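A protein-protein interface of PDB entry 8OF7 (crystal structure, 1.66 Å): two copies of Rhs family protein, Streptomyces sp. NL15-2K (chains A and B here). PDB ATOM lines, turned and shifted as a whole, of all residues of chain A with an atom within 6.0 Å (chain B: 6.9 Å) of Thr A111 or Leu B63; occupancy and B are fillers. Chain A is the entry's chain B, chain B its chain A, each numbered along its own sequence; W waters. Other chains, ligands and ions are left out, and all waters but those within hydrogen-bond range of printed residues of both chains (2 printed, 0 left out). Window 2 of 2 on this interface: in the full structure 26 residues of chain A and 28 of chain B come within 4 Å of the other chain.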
ATOM      1  N   GLN A  79      23.264   3.745  -4.992  1.00  0.00           N
ATOM      2  CA  GLN A  79      22.200   3.571  -5.954  1.00  0.00           C
ATOM      3  C   GLN A  79      20.908   3.984  -5.296  1.00  0.00           C
ATOM      4  O   GLN A  79      20.657   3.571  -4.169  1.00  0.00           O
ATOM      5  CB  GLN A  79      22.170   2.145  -6.493  1.00  0.00           C
ATOM      6  CG  GLN A  79      23.533   1.776  -7.083  1.00  0.00           C
ATOM      7  CD  GLN A  79      23.443   0.523  -7.927  1.00  0.00           C
ATOM      8  OE1 GLN A  79      23.038   0.563  -9.077  1.00  0.00           O
ATOM      9  NE2 GLN A  79      23.815  -0.604  -7.360  1.00  0.00           N
ATOM     10  N   ILE A  80      20.112   4.710  -6.079  1.00  0.00           N
ATOM     11  CA  ILE A  80      18.859   5.236  -5.597  1.00  0.00           C
ATOM     12  C   ILE A  80      17.767   4.688  -6.478  1.00  0.00           C
ATOM     13  O   ILE A  80      17.859   4.827  -7.699  1.00  0.00           O
ATOM     14  CB  ILE A  80      18.886   6.777  -5.619  1.00  0.00           C
ATOM     15  CG1 ILE A  80      20.087   7.344  -4.866  1.00  0.00           C
ATOM     16  CG2 ILE A  80      17.565   7.320  -5.073  1.00  0.00           C
ATOM     17  CD1 ILE A  80      21.227   7.842  -5.731  1.00  0.00           C
ATOM     18  N   ARG A  81      16.746   4.112  -5.841  1.00  0.00           N
ATOM     19  CA  ARG A  81      15.591   3.583  -6.538  1.00  0.00           C
ATOM     20  C   ARG A  81      14.394   4.480  -6.257  1.00  0.00           C
ATOM     21  O   ARG A  81      14.126   4.756  -5.091  1.00  0.00           O
ATOM     22  CB  ARG A  81      15.294   2.156  -6.062  1.00  0.00           C
ATOM     23  CG  ARG A  81      13.964   1.593  -6.544  1.00  0.00           C
ATOM     24  CD  ARG A  81      13.824   0.092  -6.269  1.00  0.00           C
ATOM     25  NE  ARG A  81      13.397  -0.505  -7.521  1.00  0.00           N
ATOM     26  CZ  ARG A  81      14.205  -1.123  -8.359  1.00  0.00           C
ATOM     27  NH1 ARG A  81      13.904  -1.163  -9.647  1.00  0.00           N
ATOM     28  NH2 ARG A  81      15.361  -1.599  -7.928  1.00  0.00           N
ATOM     29  N   THR A  86      16.001   4.465 -11.721  1.00  0.00           N
ATOM     30  CA  THR A  86      17.103   4.216 -10.811  1.00  0.00           C
ATOM     31  C   THR A  86      18.267   5.078 -11.273  1.00  0.00           C
ATOM     32  O   THR A  86      18.416   5.359 -12.468  1.00  0.00           O
ATOM     33  CB  THR A  86      17.508   2.723 -10.758  1.00  0.00           C
ATOM     34  OG1 THR A  86      17.910   2.369 -12.084  1.00  0.00           O
ATOM     35  CG2 THR A  86      16.399   1.802 -10.274  1.00  0.00           C
ATOM     36  N   ILE A  87      19.083   5.467 -10.296  1.00  0.00           N
ATOM     37  CA  ILE A  87      20.221   6.353 -10.474  1.00  0.00           C
ATOM     38  C   ILE A  87      21.398   5.810  -9.657  1.00  0.00           C
ATOM     39  O   ILE A  87      21.254   5.353  -8.524  1.00  0.00           O
ATOM     40  CB  ILE A  87      19.849   7.780  -9.983  1.00  0.00           C
ATOM     41  CG1 ILE A  87      18.689   8.364 -10.791  1.00  0.00           C
ATOM     42  CG2 ILE A  87      21.037   8.733 -10.016  1.00  0.00           C
ATOM     43  CD1 ILE A  87      18.033   9.584 -10.160  1.00  0.00           C
ATOM     44  N   MET A  88      22.588   5.900 -10.214  1.00  0.00           N
ATOM     45  CA  MET A  88      23.811   5.654  -9.468  1.00  0.00           C
ATOM     46  C   MET A  88      24.497   6.997  -9.210  1.00  0.00           C
ATOM     47  O   MET A  88      24.523   7.838 -10.104  1.00  0.00           O
ATOM     48  CB  MET A  88      24.757   4.757 -10.266  1.00  0.00           C
ATOM     49  CG  MET A  88      26.134   4.572  -9.586  1.00  0.00           C
ATOM     50  SD  MET A  88      27.247   3.559 -10.646  1.00  0.00           S
ATOM     51  CE  MET A  88      28.832   3.897  -9.873  1.00  0.00           C
ATOM     52  N   GLN A 109      24.375   9.334 -12.588  1.00  0.00           N
ATOM     53  CA  GLN A 109      24.005   8.830 -13.910  1.00  0.00           C
ATOM     54  C   GLN A 109      22.759   7.982 -13.729  1.00  0.00           C
ATOM     55  O   GLN A 109      22.685   7.129 -12.825  1.00  0.00           O
ATOM     56  CB  GLN A 109      25.196   8.026 -14.429  1.00  0.00           C
ATOM     57  CG  GLN A 109      24.948   7.279 -15.713  1.00  0.00           C
ATOM     58  CD  GLN A 109      26.153   6.430 -16.035  1.00  0.00           C
ATOM     59  OE1 GLN A 109      26.562   5.557 -15.261  1.00  0.00           O
ATOM     60  NE2 GLN A 109      26.745   6.715 -17.185  1.00  0.00           N
ATOM     61  N   GLY A 110      21.754   8.242 -14.548  1.00  0.00           N
ATOM     62  CA  GLY A 110      20.595   7.364 -14.574  1.00  0.00           C
ATOM     63  C   GLY A 110      20.958   5.964 -15.073  1.00  0.00           C
ATOM     64  O   GLY A 110      21.783   5.816 -15.955  1.00  0.00           O
ATOM     65  N   THR A 111      20.396   4.945 -14.423  1.00  0.00           N
ATOM     66  CA  THR A 111      20.681   3.564 -14.783  1.00  0.00           C
ATOM     67  C   THR A 111      19.458   2.898 -15.389  1.00  0.00           C
ATOM     68  O   THR A 111      19.614   1.880 -16.028  1.00  0.00           O
ATOM     69  CB  THR A 111      21.238   2.761 -13.596  1.00  0.00           C
ATOM     70  OG1 THR A 111      20.412   2.929 -12.437  1.00  0.00           O
ATOM     71  CG2 THR A 111      22.681   3.127 -13.318  1.00  0.00           C
ATOM     72  N   SER A 112      18.250   3.373 -15.121  1.00  0.00           N
ATOM     73  CA  SER A 112      17.100   2.781 -15.793  1.00  0.00           C
ATOM     74  C   SER A 112      15.918   3.737 -15.717  1.00  0.00           C
ATOM     75  O   SER A 112      15.955   4.718 -14.960  1.00  0.00           O
ATOM     76  CB  SER A 112      16.714   1.450 -15.147  1.00  0.00           C
ATOM     77  OG  SER A 112      16.146   1.652 -13.846  1.00  0.00           O
ATOM     78  N   GLY A 113      14.832   3.347 -16.385  1.00  0.00           N
ATOM     79  CA  GLY A 113      13.580   4.091 -16.416  1.00  0.00           C
ATOM     80  C   GLY A 113      13.768   5.519 -16.939  1.00  0.00           C
ATOM     81  O   GLY A 113      14.606   5.777 -17.814  1.00  0.00           O
ATOM     82  N   TYR A 115      15.328   7.976 -15.986  1.00  0.00           N
ATOM     83  CA  TYR A 115      16.656   8.576 -15.854  1.00  0.00           C
ATOM     84  C   TYR A 115      17.676   7.977 -16.809  1.00  0.00           C
ATOM     85  O   TYR A 115      18.849   8.399 -16.815  1.00  0.00           O
ATOM     86  CB  TYR A 115      17.120   8.490 -14.398  1.00  0.00           C
ATOM     87  CG  TYR A 115      16.042   8.981 -13.461  1.00  0.00           C
ATOM     88  CD1 TYR A 115      15.671  10.327 -13.428  1.00  0.00           C
ATOM     89  CD2 TYR A 115      15.293   8.099 -12.708  1.00  0.00           C
ATOM     90  CE1 TYR A 115      14.612  10.772 -12.649  1.00  0.00           C
ATOM     91  CE2 TYR A 115      14.258   8.531 -11.896  1.00  0.00           C
ATOM     92  CZ  TYR A 115      13.898   9.870 -11.885  1.00  0.00           C
ATOM     93  OH  TYR A 115      12.861  10.267 -11.073  1.00  0.00           O
ATOM     94  N   ALA A 116      17.269   6.987 -17.611  1.00  0.00           N
ATOM     95  CA  ALA A 116      18.256   6.250 -18.392  1.00  0.00           C
ATOM     96  C   ALA A 116      18.993   7.192 -19.337  1.00  0.00           C
ATOM     97  O   ALA A 116      18.370   7.960 -20.050  1.00  0.00           O
ATOM     98  CB  ALA A 116      17.572   5.172 -19.224  1.00  0.00           C
ATOM     99  N   GLY A 117      20.321   7.108 -19.393  1.00  0.00           N
ATOM    100  CA  GLY A 117      21.038   7.954 -20.320  1.00  0.00           C
ATOM    101  C   GLY A 117      21.367   9.343 -19.758  1.00  0.00           C
ATOM    102  O   GLY A 117      22.215  10.020 -20.317  1.00  0.00           O
ATOM    103  N   LEU A 118      20.697   9.777 -18.687  1.00  0.00           N
ATOM    104  CA  LEU A 118      20.872  11.126 -18.184  1.00  0.00           C
ATOM    105  C   LEU A 118      22.033  11.130 -17.200  1.00  0.00           C
ATOM    106  O   LEU A 118      22.280  10.124 -16.527  1.00  0.00           O
ATOM    107  CB  LEU A 118      19.588  11.588 -17.494  1.00  0.00           C
ATOM    108  CG  LEU A 118      18.329  11.504 -18.342  1.00  0.00           C
ATOM    109  CD1 LEU A 118      17.138  12.043 -17.573  1.00  0.00           C
ATOM    110  CD2 LEU A 118      18.500  12.251 -19.660  1.00  0.00           C
ATOM    111  N   MET B  37      15.153  -6.988  -4.524  1.00  0.00           N
ATOM    112  CA  MET B  37      15.195  -5.849  -5.428  1.00  0.00           C
ATOM    113  C   MET B  37      16.507  -5.064  -5.250  1.00  0.00           C
ATOM    114  O   MET B  37      17.023  -4.455  -6.191  1.00  0.00           O
ATOM    115  CB  MET B  37      13.983  -4.944  -5.193  1.00  0.00           C
ATOM    116  CG  MET B  37      12.695  -5.618  -5.625  1.00  0.00           C
ATOM    117  SD  MET B  37      12.645  -5.776  -7.451  1.00  0.00           S
ATOM    118  CE  MET B  37      12.567  -4.056  -7.960  1.00  0.00           C
ATOM    119  N   MET B  60      23.619  -3.386  -4.856  1.00  0.00           N
ATOM    120  CA  MET B  60      22.989  -3.939  -6.052  1.00  0.00           C
ATOM    121  C   MET B  60      21.592  -3.399  -6.107  1.00  0.00           C
ATOM    122  O   MET B  60      20.943  -3.266  -5.084  1.00  0.00           O
ATOM    123  CB  MET B  60      22.996  -5.475  -5.951  1.00  0.00           C
ATOM    124  CG  MET B  60      22.263  -6.224  -7.059  1.00  0.00           C
ATOM    125  SD  MET B  60      20.460  -6.201  -7.022  1.00  0.00           S
ATOM    126  CE  MET B  60      20.115  -7.409  -5.746  1.00  0.00           C
ATOM    127  N   ASP B  61      21.101  -3.164  -7.332  1.00  0.00           N
ATOM    128  CA  ASP B  61      19.736  -2.773  -7.589  1.00  0.00           C
ATOM    129  C   ASP B  61      19.266  -3.551  -8.833  1.00  0.00           C
ATOM    130  O   ASP B  61      20.000  -3.636  -9.824  1.00  0.00           O
ATOM    131  CB  ASP B  61      19.781  -1.278  -7.878  1.00  0.00           C
ATOM    132  CG  ASP B  61      18.531  -0.460  -7.697  1.00  0.00           C
ATOM    133  OD1 ASP B  61      17.553  -1.023  -7.215  1.00  0.00           O
ATOM    134  OD2 ASP B  61      18.573   0.759  -8.080  1.00  0.00           O
ATOM    135  N   ILE B  62      18.078  -4.132  -8.783  1.00  0.00           N
ATOM    136  CA  ILE B  62      17.462  -4.698  -9.972  1.00  0.00           C
ATOM    137  C   ILE B  62      17.009  -3.558 -10.872  1.00  0.00           C
ATOM    138  O   ILE B  62      16.369  -2.603 -10.427  1.00  0.00           O
ATOM    139  CB  ILE B  62      16.280  -5.622  -9.625  1.00  0.00           C
ATOM    140  CG1 ILE B  62      16.769  -6.918  -8.977  1.00  0.00           C
ATOM    141  CG2 ILE B  62      15.444  -5.950 -10.859  1.00  0.00           C
ATOM    142  CD1 ILE B  62      15.668  -7.927  -8.731  1.00  0.00           C
ATOM    143  N   LEU B  63      17.374  -3.631 -12.148  1.00  0.00           N
ATOM    144  CA  LEU B  63      16.913  -2.632 -13.093  1.00  0.00           C
ATOM    145  C   LEU B  63      15.570  -3.070 -13.664  1.00  0.00           C
ATOM    146  O   LEU B  63      14.608  -2.329 -13.660  1.00  0.00           O
ATOM    147  CB  LEU B  63      17.937  -2.444 -14.202  1.00  0.00           C
ATOM    148  CG  LEU B  63      19.299  -1.986 -13.724  1.00  0.00           C
ATOM    149  CD1 LEU B  63      20.200  -1.654 -14.904  1.00  0.00           C
ATOM    150  CD2 LEU B  63      19.169  -0.801 -12.766  1.00  0.00           C
ATOM    151  N   TYR B  64      15.536  -4.289 -14.197  1.00  0.00           N
ATOM    152  CA  TYR B  64      14.327  -4.749 -14.861  1.00  0.00           C
ATOM    153  C   TYR B  64      14.509  -6.214 -15.212  1.00  0.00           C
ATOM    154  O   TYR B  64      15.581  -6.764 -15.076  1.00  0.00           O
ATOM    155  CB  TYR B  64      14.082  -3.891 -16.098  1.00  0.00           C
ATOM    156  CG  TYR B  64      15.281  -3.737 -16.992  1.00  0.00           C
ATOM    157  CD1 TYR B  64      15.656  -4.761 -17.832  1.00  0.00           C
ATOM    158  CD2 TYR B  64      15.990  -2.551 -17.049  1.00  0.00           C
ATOM    159  CE1 TYR B  64      16.729  -4.643 -18.694  1.00  0.00           C
ATOM    160  CE2 TYR B  64      17.105  -2.426 -17.884  1.00  0.00           C
ATOM    161  CZ  TYR B  64      17.485  -3.489 -18.676  1.00  0.00           C
ATOM    162  OH  TYR B  64      18.508  -3.423 -19.573  1.00  0.00           O
ATOM    163  N   ALA B  65      13.436  -6.844 -15.657  1.00  0.00           N
ATOM    164  CA  ALA B  65      13.503  -8.133 -16.345  1.00  0.00           C
ATOM    165  C   ALA B  65      13.601  -7.878 -17.858  1.00  0.00           C
ATOM    166  O   ALA B  65      12.910  -7.014 -18.406  1.00  0.00           O
ATOM    167  CB  ALA B  65      12.249  -8.964 -16.102  1.00  0.00           C
ATOM    168  N   LEU B  72      16.680 -11.499 -15.107  1.00  0.00           N
ATOM    169  CA  LEU B  72      16.852 -10.278 -14.314  1.00  0.00           C
ATOM    170  C   LEU B  72      18.144  -9.585 -14.677  1.00  0.00           C
ATOM    171  O   LEU B  72      19.205 -10.214 -14.841  1.00  0.00           O
ATOM    172  CB  LEU B  72      16.838 -10.657 -12.840  1.00  0.00           C
ATOM    173  CG  LEU B  72      15.549 -11.241 -12.294  1.00  0.00           C
ATOM    174  CD1 LEU B  72      15.673 -11.482 -10.762  1.00  0.00           C
ATOM    175  CD2 LEU B  72      14.373 -10.325 -12.577  1.00  0.00           C
ATOM    176  N   VAL B  73      18.004  -8.273 -14.867  1.00  0.00           N
ATOM    177  CA  VAL B  73      19.147  -7.431 -15.121  1.00  0.00           C
ATOM    178  C   VAL B  73      19.335  -6.558 -13.877  1.00  0.00           C
ATOM    179  O   VAL B  73      18.429  -5.800 -13.448  1.00  0.00           O
ATOM    180  CB  VAL B  73      18.976  -6.570 -16.391  1.00  0.00           C
ATOM    181  CG1 VAL B  73      20.161  -5.622 -16.618  1.00  0.00           C
ATOM    182  CG2 VAL B  73      18.717  -7.445 -17.620  1.00  0.00           C
ATOM    183  N   GLU B  74      20.562  -6.571 -13.393  1.00  0.00           N
ATOM    184  CA  GLU B  74      20.911  -5.901 -12.153  1.00  0.00           C
ATOM    185  C   GLU B  74      22.080  -4.956 -12.399  1.00  0.00           C
ATOM    186  O   GLU B  74      22.843  -5.127 -13.344  1.00  0.00           O
ATOM    187  CB  GLU B  74      21.402  -6.889 -11.109  1.00  0.00           C
ATOM    188  CG  GLU B  74      20.269  -7.717 -10.535  1.00  0.00           C
ATOM    189  CD  GLU B  74      20.627  -8.739  -9.451  1.00  0.00           C
ATOM    190  OE1 GLU B  74      21.860  -8.869  -9.135  1.00  0.00           O
ATOM    191  OE2 GLU B  74      19.640  -9.440  -8.985  1.00  0.00           O
ATOM    192  N   HIS B  75      22.186  -3.943 -11.524  1.00  0.00           N
ATOM    193  CA  HIS B  75      23.281  -3.002 -11.582  1.00  0.00           C
ATOM    194  C   HIS B  75      23.990  -2.972 -10.222  1.00  0.00           C
ATOM    195  O   HIS B  75      23.352  -2.938  -9.198  1.00  0.00           O
ATOM    196  CB  HIS B  75      22.751  -1.602 -11.909  1.00  0.00           C
ATOM    197  CG  HIS B  75      23.834  -0.663 -12.334  1.00  0.00           C
ATOM    198  ND1 HIS B  75      24.519   0.159 -11.460  1.00  0.00           N
ATOM    199  CD2 HIS B  75      24.418  -0.500 -13.543  1.00  0.00           C
ATOM    200  CE1 HIS B  75      25.436   0.843 -12.158  1.00  0.00           C
ATOM    201  NE2 HIS B  75      25.397   0.439 -13.427  1.00  0.00           N
ATOM    202  N   GLY B  91      28.656  -1.713 -12.869  1.00  0.00           N
ATOM    203  CA  GLY B  91      28.199  -2.249 -14.141  1.00  0.00           C
ATOM    204  C   GLY B  91      26.850  -2.941 -14.034  1.00  0.00           C
ATOM    205  O   GLY B  91      26.315  -3.180 -12.952  1.00  0.00           O
ATOM    206  N   THR B  92      26.380  -3.354 -15.208  1.00  0.00           N
ATOM    207  CA  THR B  92      25.110  -4.038 -15.328  1.00  0.00           C
ATOM    208  C   THR B  92      25.438  -5.497 -15.629  1.00  0.00           C
ATOM    209  O   THR B  92      26.388  -5.742 -16.344  1.00  0.00           O
ATOM    210  CB  THR B  92      24.330  -3.425 -16.488  1.00  0.00           C
ATOM    211  OG1 THR B  92      24.159  -2.044 -16.191  1.00  0.00           O
ATOM    212  CG2 THR B  92      22.959  -4.021 -16.692  1.00  0.00           C
ATOM    213  N   MET B  93      24.652  -6.453 -15.148  1.00  0.00           N
ATOM    214  CA  MET B  93      24.858  -7.854 -15.528  1.00  0.00           C
ATOM    215  C   MET B  93      23.514  -8.537 -15.627  1.00  0.00           C
ATOM    216  O   MET B  93      22.567  -8.140 -14.958  1.00  0.00           O
ATOM    217  CB  MET B  93      25.626  -8.600 -14.445  1.00  0.00           C
ATOM    218  CG  MET B  93      25.057  -8.285 -13.116  1.00  0.00           C
ATOM    219  SD  MET B  93      26.130  -8.689 -11.867  1.00  0.00           S
ATOM    220  CE  MET B  93      24.944  -9.127 -10.602  1.00  0.00           C
HETATM  221  O   HOH W   1      22.229   0.733 -16.782  1.00  0.00           O
HETATM  222  O   HOH W   2      26.444   2.204 -15.372  1.00  0.00           O
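Water W2 bridges a ring nitrogen (NE2) of His B75 (2.8 Å) and the side-chain amide oxygen (OE1) of Gln A109 (3.4 Å).
Water W1 lies within hydrogen-bond range of the backbone carbonyl oxygen (O) of Thr A111 (3.0 Å) and the side-chain hydroxyl (OG1) of Thr B92 (3.4 Å).
O of Ile B62 lies within hydrogen-bond range of NH2 of Arg A81, 2.9 Å away.
OE1 of Gln A79 is in hydrogen-bond range of ND1 of His B75 (2.8 Å).
The side-chain carboxylate of Asp B61 lies within salt-bridge range of the guanidinium group of Arg A81 (3.99 Å).
No position is printed for both chains.
Of the 11 pairs that touch across the chains among the printed residues, none has its exchanged pair printed and touching as well.
The side-chain hydroxyl (OG1) of Thr A86 lies within hydrogen-bond range of the side-chain hydroxyl (OG) of Ser A112, at 2.6 Å.
N of Leu B63 lies within hydrogen-bond range of O of Val B73 (2.7 Å).
The backbone carbonyl oxygen (O) of Asp B61 lies within hydrogen-bond range of the backbone NH (N) of His B75.
The backbone NH of Met A88 sits at hydrogen-bond distance from the backbone carbonyl oxygen of Gln A109 (2.9 Å).
The side-chain hydroxyl of Thr A86 sits at hydrogen-bond distance from the side-chain hydroxyl of Thr A111, 2.6 Å away.
SD of Met B60 sits at hydrogen-bond distance from N of Ile B62 (3.6 Å).
CA of Met B60 touches NE2 of Gln A79, 3.7 Å away.
NE2 of Gln A79 touches N of Asp B61 (3.7 Å).
Arg A81 touches Met B37.
OD2 of Asp B61 touches CG2 of Thr A86, 3.3 Å away.
OG1 of Thr A86 touches CD2 of Leu B63, 3.5 Å away.
CE1 of His B75 touches SD of Met A88, 3.6 Å away.
Thr A111 touches Leu B63 (O to CD1, 3.8 Å).
CE1 of His B75 touches CG2 of Thr A111, at 3.8 Å.
Of the printed residues of chain B, Gln A79 touches Met B60 (3.7 Å), Asp B61 (3.7 Å) and His B75 (2.8 Å).
Of the printed residues of chain B, Arg A81 touches Met B37 (3.4 Å), Asp B61 (2.4 Å) and Ile B62 (2.9 Å).
Thr A111 touches just these residues of chain B: Leu B63 (3.8 Å) and His B75 (3.8 Å).
Printed residues of chain A within 4 Å of Asp B61: Gln A79, Arg A81 and Thr A86.
Of the printed residues of chain A, Ile B62 touches Arg A81.
Printed residues of chain A within 4 Å of Leu B63: Thr A86 (3.5 Å) and Thr A111 (3.8 Å).
The nearest residue of chain B that does not touch Thr A111 is Asp B61 (5.2 Å).
Hydrophobic or aromatic side chains of chain A that line the printed part of chain B: Met A88.
Hydrophobic or aromatic side chains of chain B that line the printed part of chain A: Met B37, Leu B63 and His B75.
Along chain B the printed residues that touch a printed residue of chain A span positions 37 to 75.
Among the printed residues, 11 pairs touch across the chains.
Among the printed residues, Asp or Glu carboxylates within 4 Å of a Lys or Arg side-chain nitrogen of the other chain: Arg A81 with Asp B61.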
